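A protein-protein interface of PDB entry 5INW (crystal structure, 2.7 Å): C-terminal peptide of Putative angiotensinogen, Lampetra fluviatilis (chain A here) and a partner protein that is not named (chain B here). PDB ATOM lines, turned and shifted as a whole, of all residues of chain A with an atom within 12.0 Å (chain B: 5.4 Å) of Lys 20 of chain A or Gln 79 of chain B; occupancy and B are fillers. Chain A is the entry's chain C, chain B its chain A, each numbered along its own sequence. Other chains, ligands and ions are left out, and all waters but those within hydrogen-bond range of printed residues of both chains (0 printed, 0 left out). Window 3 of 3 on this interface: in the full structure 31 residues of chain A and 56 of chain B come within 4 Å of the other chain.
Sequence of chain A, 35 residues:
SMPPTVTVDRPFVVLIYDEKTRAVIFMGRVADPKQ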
ATOM      1  N   ILE A  16       7.334 -29.416 -16.048  1.00  0.00           N
ATOM      2  CA  ILE A  16       7.386 -28.005 -16.282  1.00  0.00           C
ATOM      3  C   ILE A  16       7.877 -27.882 -17.712  1.00  0.00           C
ATOM      4  O   ILE A  16       8.964 -28.375 -18.022  1.00  0.00           O
ATOM      5  CB  ILE A  16       8.350 -27.357 -15.287  1.00  0.00           C
ATOM      6  CG1 ILE A  16       7.739 -27.364 -13.904  1.00  0.00           C
ATOM      7  CG2 ILE A  16       8.654 -25.930 -15.698  1.00  0.00           C
ATOM      8  CD1 ILE A  16       8.702 -27.005 -12.817  1.00  0.00           C
ATOM      9  N   TYR A  17       7.106 -27.236 -18.585  1.00  0.00           N
ATOM     10  CA  TYR A  17       7.424 -27.267 -20.010  1.00  0.00           C
ATOM     11  C   TYR A  17       7.087 -25.980 -20.747  1.00  0.00           C
ATOM     12  O   TYR A  17       6.221 -25.233 -20.326  1.00  0.00           O
ATOM     13  CB  TYR A  17       6.676 -28.440 -20.642  1.00  0.00           C
ATOM     14  CG  TYR A  17       5.203 -28.178 -20.792  1.00  0.00           C
ATOM     15  CD1 TYR A  17       4.304 -28.309 -19.702  1.00  0.00           C
ATOM     16  CD2 TYR A  17       4.699 -27.744 -22.016  1.00  0.00           C
ATOM     17  CE1 TYR A  17       2.942 -28.030 -19.866  1.00  0.00           C
ATOM     18  CE2 TYR A  17       3.350 -27.467 -22.182  1.00  0.00           C
ATOM     19  CZ  TYR A  17       2.466 -27.600 -21.127  1.00  0.00           C
ATOM     20  OH  TYR A  17       1.126 -27.277 -21.390  1.00  0.00           O
ATOM     21  N   ASP A  18       7.780 -25.720 -21.841  1.00  0.00           N
ATOM     22  CA  ASP A  18       7.505 -24.547 -22.674  1.00  0.00           C
ATOM     23  C   ASP A  18       6.424 -24.940 -23.615  1.00  0.00           C
ATOM     24  O   ASP A  18       6.527 -25.992 -24.255  1.00  0.00           O
ATOM     25  CB  ASP A  18       8.744 -24.152 -23.482  1.00  0.00           C
ATOM     26  CG  ASP A  18       8.494 -23.031 -24.470  1.00  0.00           C
ATOM     27  OD1 ASP A  18       7.631 -22.144 -24.253  1.00  0.00           O
ATOM     28  OD2 ASP A  18       9.162 -23.069 -25.514  1.00  0.00           O
ATOM     29  N   GLU A  19       5.419 -24.081 -23.755  1.00  0.00           N
ATOM     30  CA  GLU A  19       4.300 -24.359 -24.645  1.00  0.00           C
ATOM     31  C   GLU A  19       4.666 -24.344 -26.114  1.00  0.00           C
ATOM     32  O   GLU A  19       4.382 -25.316 -26.760  1.00  0.00           O
ATOM     33  CB  GLU A  19       3.149 -23.425 -24.379  1.00  0.00           C
ATOM     34  CG  GLU A  19       2.548 -23.697 -23.024  1.00  0.00           C
ATOM     35  CD  GLU A  19       1.799 -22.523 -22.489  1.00  0.00           C
ATOM     36  OE1 GLU A  19       1.225 -21.764 -23.298  1.00  0.00           O
ATOM     37  OE2 GLU A  19       1.786 -22.343 -21.247  1.00  0.00           O
ATOM     38  N   LYS A  20       5.314 -23.297 -26.633  1.00  0.00           N
ATOM     39  CA  LYS A  20       5.629 -23.226 -28.076  1.00  0.00           C
ATOM     40  C   LYS A  20       6.465 -24.403 -28.491  1.00  0.00           C
ATOM     41  O   LYS A  20       6.087 -25.102 -29.410  1.00  0.00           O
ATOM     42  CB  LYS A  20       6.356 -21.954 -28.481  1.00  0.00           C
ATOM     43  CG  LYS A  20       5.498 -20.702 -28.399  1.00  0.00           C
ATOM     44  CD  LYS A  20       6.340 -19.402 -28.462  1.00  0.00           C
ATOM     45  CE  LYS A  20       5.714 -18.244 -27.673  1.00  0.00           C
ATOM     46  NZ  LYS A  20       5.855 -18.302 -26.179  1.00  0.00           N
ATOM     47  N   THR A  21       7.583 -24.660 -27.815  1.00  0.00           N
ATOM     48  CA  THR A  21       8.463 -25.804 -28.201  1.00  0.00           C
ATOM     49  C   THR A  21       8.109 -27.183 -27.614  1.00  0.00           C
ATOM     50  O   THR A  21       8.708 -28.167 -27.981  1.00  0.00           O
ATOM     51  CB  THR A  21       9.947 -25.494 -27.892  1.00  0.00           C
ATOM     52  OG1 THR A  21      10.142 -25.370 -26.487  1.00  0.00           O
ATOM     53  CG2 THR A  21      10.359 -24.210 -28.550  1.00  0.00           C
ATOM     54  N   ARG A  22       7.147 -27.245 -26.700  1.00  0.00           N
ATOM     55  CA  ARG A  22       6.866 -28.442 -25.903  1.00  0.00           C
ATOM     56  C   ARG A  22       8.113 -29.035 -25.254  1.00  0.00           C
ATOM     57  O   ARG A  22       8.189 -30.224 -25.008  1.00  0.00           O
ATOM     58  CB  ARG A  22       6.060 -29.459 -26.701  1.00  0.00           C
ATOM     59  CG  ARG A  22       4.592 -29.022 -26.789  1.00  0.00           C
ATOM     60  CD  ARG A  22       3.849 -29.606 -27.983  1.00  0.00           C
ATOM     61  NE  ARG A  22       2.724 -28.824 -28.516  1.00  0.00           N
ATOM     62  CZ  ARG A  22       1.967 -29.243 -29.546  1.00  0.00           C
ATOM     63  NH1 ARG A  22       2.193 -30.440 -30.129  1.00  0.00           N
ATOM     64  NH2 ARG A  22       0.960 -28.477 -29.999  1.00  0.00           N
ATOM     65  N   ALA A  23       9.059 -28.158 -24.909  1.00  0.00           N
ATOM     66  CA  ALA A  23      10.313 -28.575 -24.304  1.00  0.00           C
ATOM     67  C   ALA A  23      10.080 -28.773 -22.834  1.00  0.00           C
ATOM     68  O   ALA A  23       9.643 -27.856 -22.117  1.00  0.00           O
ATOM     69  CB  ALA A  23      11.408 -27.537 -24.513  1.00  0.00           C
ATOM     70  N   VAL A  24      10.408 -29.970 -22.369  1.00  0.00           N
ATOM     71  CA  VAL A  24      10.316 -30.263 -20.966  1.00  0.00           C
ATOM     72  C   VAL A  24      11.617 -29.882 -20.301  1.00  0.00           C
ATOM     73  O   VAL A  24      12.696 -30.350 -20.665  1.00  0.00           O
ATOM     74  CB  VAL A  24      10.008 -31.706 -20.732  1.00  0.00           C
ATOM     75  CG1 VAL A  24       9.965 -31.963 -19.230  1.00  0.00           C
ATOM     76  CG2 VAL A  24       8.699 -32.005 -21.395  1.00  0.00           C
ATOM     77  N   ILE A  25      11.471 -29.060 -19.286  1.00  0.00           N
ATOM     78  CA  ILE A  25      12.563 -28.442 -18.606  1.00  0.00           C
ATOM     79  C   ILE A  25      12.878 -29.154 -17.302  1.00  0.00           C
ATOM     80  O   ILE A  25      14.045 -29.241 -16.945  1.00  0.00           O
ATOM     81  CB  ILE A  25      12.204 -26.973 -18.325  1.00  0.00           C
ATOM     82  CG1 ILE A  25      11.809 -26.314 -19.639  1.00  0.00           C
ATOM     83  CG2 ILE A  25      13.380 -26.213 -17.698  1.00  0.00           C
ATOM     84  CD1 ILE A  25      11.208 -24.965 -19.445  1.00  0.00           C
ATOM     85  N   LYS B  74       7.255 -32.746 -33.443  1.00  0.00           N
ATOM     86  CA  LYS B  74       6.410 -31.991 -34.422  1.00  0.00           C
ATOM     87  C   LYS B  74       7.213 -31.088 -35.377  1.00  0.00           C
ATOM     88  O   LYS B  74       8.276 -30.583 -35.024  1.00  0.00           O
ATOM     89  CB  LYS B  74       5.311 -31.181 -33.707  1.00  0.00           C
ATOM     90  CG  LYS B  74       4.185 -32.050 -33.165  1.00  0.00           C
ATOM     91  CD  LYS B  74       2.821 -31.645 -33.714  1.00  0.00           C
ATOM     92  CE  LYS B  74       1.784 -32.716 -33.416  1.00  0.00           C
ATOM     93  NZ  LYS B  74       0.433 -32.124 -33.291  1.00  0.00           N
ATOM     94  N   LYS B  75       6.659 -30.915 -36.581  1.00  0.00           N
ATOM     95  CA  LYS B  75       7.306 -30.227 -37.740  1.00  0.00           C
ATOM     96  C   LYS B  75       8.533 -29.251 -37.524  1.00  0.00           C
ATOM     97  O   LYS B  75       9.497 -29.327 -38.273  1.00  0.00           O
ATOM     98  CB  LYS B  75       6.245 -29.526 -38.640  1.00  0.00           C
ATOM     99  CG  LYS B  75       4.964 -30.297 -38.929  1.00  0.00           C
ATOM    100  CD  LYS B  75       3.885 -29.810 -37.971  1.00  0.00           C
ATOM    101  CE  LYS B  75       2.654 -30.683 -38.058  1.00  0.00           C
ATOM    102  NZ  LYS B  75       1.467 -29.949 -37.553  1.00  0.00           N
ATOM    103  N   SER B  76       8.502 -28.345 -36.552  1.00  0.00           N
ATOM    104  CA  SER B  76       9.506 -27.262 -36.456  1.00  0.00           C
ATOM    105  C   SER B  76      10.890 -27.771 -36.095  1.00  0.00           C
ATOM    106  O   SER B  76      11.002 -28.825 -35.508  1.00  0.00           O
ATOM    107  CB  SER B  76       9.099 -26.251 -35.385  1.00  0.00           C
ATOM    108  OG  SER B  76      10.098 -25.256 -35.178  1.00  0.00           O
ATOM    109  N   LYS B  77      11.939 -27.001 -36.385  1.00  0.00           N
ATOM    110  CA  LYS B  77      13.331 -27.466 -36.125  1.00  0.00           C
ATOM    111  C   LYS B  77      13.563 -27.544 -34.598  1.00  0.00           C
ATOM    112  O   LYS B  77      13.939 -28.584 -34.085  1.00  0.00           O
ATOM    113  CB  LYS B  77      14.407 -26.579 -36.824  1.00  0.00           C
ATOM    114  CG  LYS B  77      14.426 -26.631 -38.361  1.00  0.00           C
ATOM    115  CD  LYS B  77      13.430 -25.666 -39.032  1.00  0.00           C
ATOM    116  CE  LYS B  77      13.490 -25.716 -40.551  1.00  0.00           C
ATOM    117  NZ  LYS B  77      12.250 -25.110 -41.097  1.00  0.00           N
ATOM    118  N   THR B  78      13.283 -26.441 -33.893  1.00  0.00           N
ATOM    119  CA  THR B  78      13.386 -26.373 -32.422  1.00  0.00           C
ATOM    120  C   THR B  78      12.544 -27.429 -31.703  1.00  0.00           C
ATOM    121  O   THR B  78      12.972 -27.989 -30.707  1.00  0.00           O
ATOM    122  CB  THR B  78      12.978 -24.971 -31.908  1.00  0.00           C
ATOM    123  OG1 THR B  78      11.784 -24.541 -32.574  1.00  0.00           O
ATOM    124  CG2 THR B  78      14.097 -23.965 -32.148  1.00  0.00           C
ATOM    125  N   GLN B  79      11.356 -27.697 -32.241  1.00  0.00           N
ATOM    126  CA  GLN B  79      10.461 -28.735 -31.715  1.00  0.00           C
ATOM    127  C   GLN B  79      11.019 -30.165 -31.813  1.00  0.00           C
ATOM    128  O   GLN B  79      10.844 -30.928 -30.878  1.00  0.00           O
ATOM    129  CB  GLN B  79       9.084 -28.655 -32.372  1.00  0.00           C
ATOM    130  CG  GLN B  79       8.344 -27.388 -31.949  1.00  0.00           C
ATOM    131  CD  GLN B  79       7.083 -27.092 -32.746  1.00  0.00           C
ATOM    132  OE1 GLN B  79       6.875 -27.630 -33.825  1.00  0.00           O
ATOM    133  NE2 GLN B  79       6.259 -26.193 -32.232  1.00  0.00           N
ATOM    134  N   ARG B  80      11.716 -30.496 -32.906  1.00  0.00           N
ATOM    135  CA  ARG B  80      12.373 -31.803 -33.074  1.00  0.00           C
ATOM    136  C   ARG B  80      13.466 -32.056 -32.056  1.00  0.00           C
ATOM    137  O   ARG B  80      13.534 -33.140 -31.473  1.00  0.00           O
ATOM    138  CB  ARG B  80      12.949 -31.994 -34.485  1.00  0.00           C
ATOM    139  CG  ARG B  80      11.873 -32.166 -35.584  1.00  0.00           C
ATOM    140  CD  ARG B  80      12.423 -32.618 -36.955  1.00  0.00           C
ATOM    141  NE  ARG B  80      11.681 -32.047 -38.087  1.00  0.00           N
ATOM    142  CZ  ARG B  80      12.079 -31.044 -38.893  1.00  0.00           C
ATOM    143  NH1 ARG B  80      13.256 -30.421 -38.757  1.00  0.00           N
ATOM    144  NH2 ARG B  80      11.268 -30.641 -39.878  1.00  0.00           N
ATOM    145  N   ILE B  81      14.324 -31.070 -31.855  1.00  0.00           N
ATOM    146  CA  ILE B  81      15.398 -31.177 -30.854  1.00  0.00           C
ATOM    147  C   ILE B  81      14.854 -31.156 -29.410  1.00  0.00           C
ATOM    148  O   ILE B  81      15.386 -31.845 -28.538  1.00  0.00           O
ATOM    149  CB  ILE B  81      16.531 -30.148 -31.101  1.00  0.00           C
ATOM    150  CG1 ILE B  81      17.655 -30.240 -30.046  1.00  0.00           C
ATOM    151  CG2 ILE B  81      15.986 -28.739 -31.134  1.00  0.00           C
ATOM    152  CD1 ILE B  81      18.379 -31.585 -29.985  1.00  0.00           C
ATOM    153  N   ALA B  82      13.771 -30.417 -29.176  1.00  0.00           N
ATOM    154  CA  ALA B  82      13.100 -30.418 -27.887  1.00  0.00           C
ATOM    155  C   ALA B  82      12.566 -31.817 -27.543  1.00  0.00           C
ATOM    156  O   ALA B  82      12.652 -32.266 -26.403  1.00  0.00           O
ATOM    157  CB  ALA B  82      11.977 -29.384 -27.876  1.00  0.00           C
ATOM    158  N   SER B  83      12.040 -32.523 -28.543  1.00  0.00           N
ATOM    159  CA  SER B  83      11.506 -33.906 -28.332  1.00  0.00           C
ATOM    160  C   SER B  83      12.591 -34.949 -28.212  1.00  0.00           C
ATOM    161  O   SER B  83      12.355 -35.960 -27.593  1.00  0.00           O
ATOM    162  CB  SER B  83      10.568 -34.325 -29.452  1.00  0.00           C
ATOM    163  OG  SER B  83      11.145 -33.944 -30.682  1.00  0.00           O
ATOM    164  N   ALA B  84      13.755 -34.694 -28.815  1.00  0.00           N
ATOM    165  CA  ALA B  84      14.930 -35.510 -28.611  1.00  0.00           C
ATOM    166  C   ALA B  84      15.352 -35.427 -27.189  1.00  0.00           C
ATOM    167  O   ALA B  84      15.646 -36.443 -26.580  1.00  0.00           O
ATOM    168  CB  ALA B  84      16.085 -35.069 -29.503  1.00  0.00           C
ATOM    169  N   GLY B 305       5.636 -18.491 -21.501  1.00  0.00           N
ATOM    170  CA  GLY B 305       4.763 -19.389 -22.278  1.00  0.00           C
ATOM    171  C   GLY B 305       4.807 -20.774 -21.722  1.00  0.00           C
ATOM    172  O   GLY B 305       4.803 -21.740 -22.468  1.00  0.00           O
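Hydrophobic or aromatic side chains of chain A that line the printed part of chain B: Ala 23. Among the printed residues, no Asp or Glu carboxylate lies within 4 Å of a Lys or Arg side-chain nitrogen of the other chain.
The side-chain amide nitrogen (NE2) of Gln 79 of chain B lies within hydrogen-bond range of the backbone carbonyl oxygen (O) of Lys 20 of chain A. The backbone NH (N) of Glu 19 of chain A sits at hydrogen-bond distance from the backbone carbonyl oxygen (O) of Gly 305 of chain B (2.7 Å). The side-chain carboxylate of Asp 18 of chain A sits close to the backbone carbonyl oxygen of Gly 305 of chain B, at 3.4 Å.
O of Lys 74 of chain B lies close to OE1 of Gln 79 of chain B, at 3.5 Å. The side-chain amide oxygen (OE1) of Gln 79 of chain B sits close to the backbone NH (N) of Ser 76 of chain B. The side-chain hydroxyl (OG) of Ser 83 of chain B lies within hydrogen-bond range of the backbone carbonyl oxygen (O) of Gln 79 of chain B (3.0 Å). OD2 of Asp 18 of chain A sits at hydrogen-bond distance from OG1 of Thr 21 of chain A (2.7 Å). The backbone NH (N) of Asp 18 of chain A sits at hydrogen-bond distance from the backbone carbonyl oxygen (O) of Ala 23 of chain A (2.8 Å). The side-chain hydroxyl (OG1) of Thr 21 of chain A sits close to the backbone NH (N) of Ala 23 of chain A, at 3.4 Å.
Of the printed residues of chain B, Asp 18 of chain A touches Gly 305. Printed residues of chain B within 4 Å of Thr 21 of chain A: Ala 82 (3.5 Å). Of the printed residues of chain B, Ala 23 of chain A touches Ala 82 (3.9 Å). Ile 25 of chain A touches none of the printed residues of chain B. Of chain A, only Arg 22 comes within 4 Å of Lys 74 of chain B. No residue of chain A comes within 4 Å of Lys 75 of chain B. No residue of chain A comes within 4 Å of Ser 76 of chain B. Lys 77 of chain B touches none of the printed residues of chain A. No residue of chain A comes within 4 Å of Thr 78 of chain B. Ile 81 of chain B touches none of the printed residues of chain A. Ala 82 of chain B touches two residues of chain A. Gly 305 of chain B touches just these residues of chain A: Asp 18 (3.4 Å) and Glu 19 (2.7 Å). The nearest residue of chain A that does not touch Gln 79 of chain B is Thr 21 of chain A (4.1 Å). The nearest printed residue of chain B that does not touch Arg 22 of chain A is Ala 82 of chain B (4.7 Å).
Among the printed residues, pairs that only touch across the chains: Thr 21 of chain A with Ala 82 of chain B, Arg 22 of chain A with Lys 74 of chain B and Ala 23 of chain A with Ala 82 of chain B.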
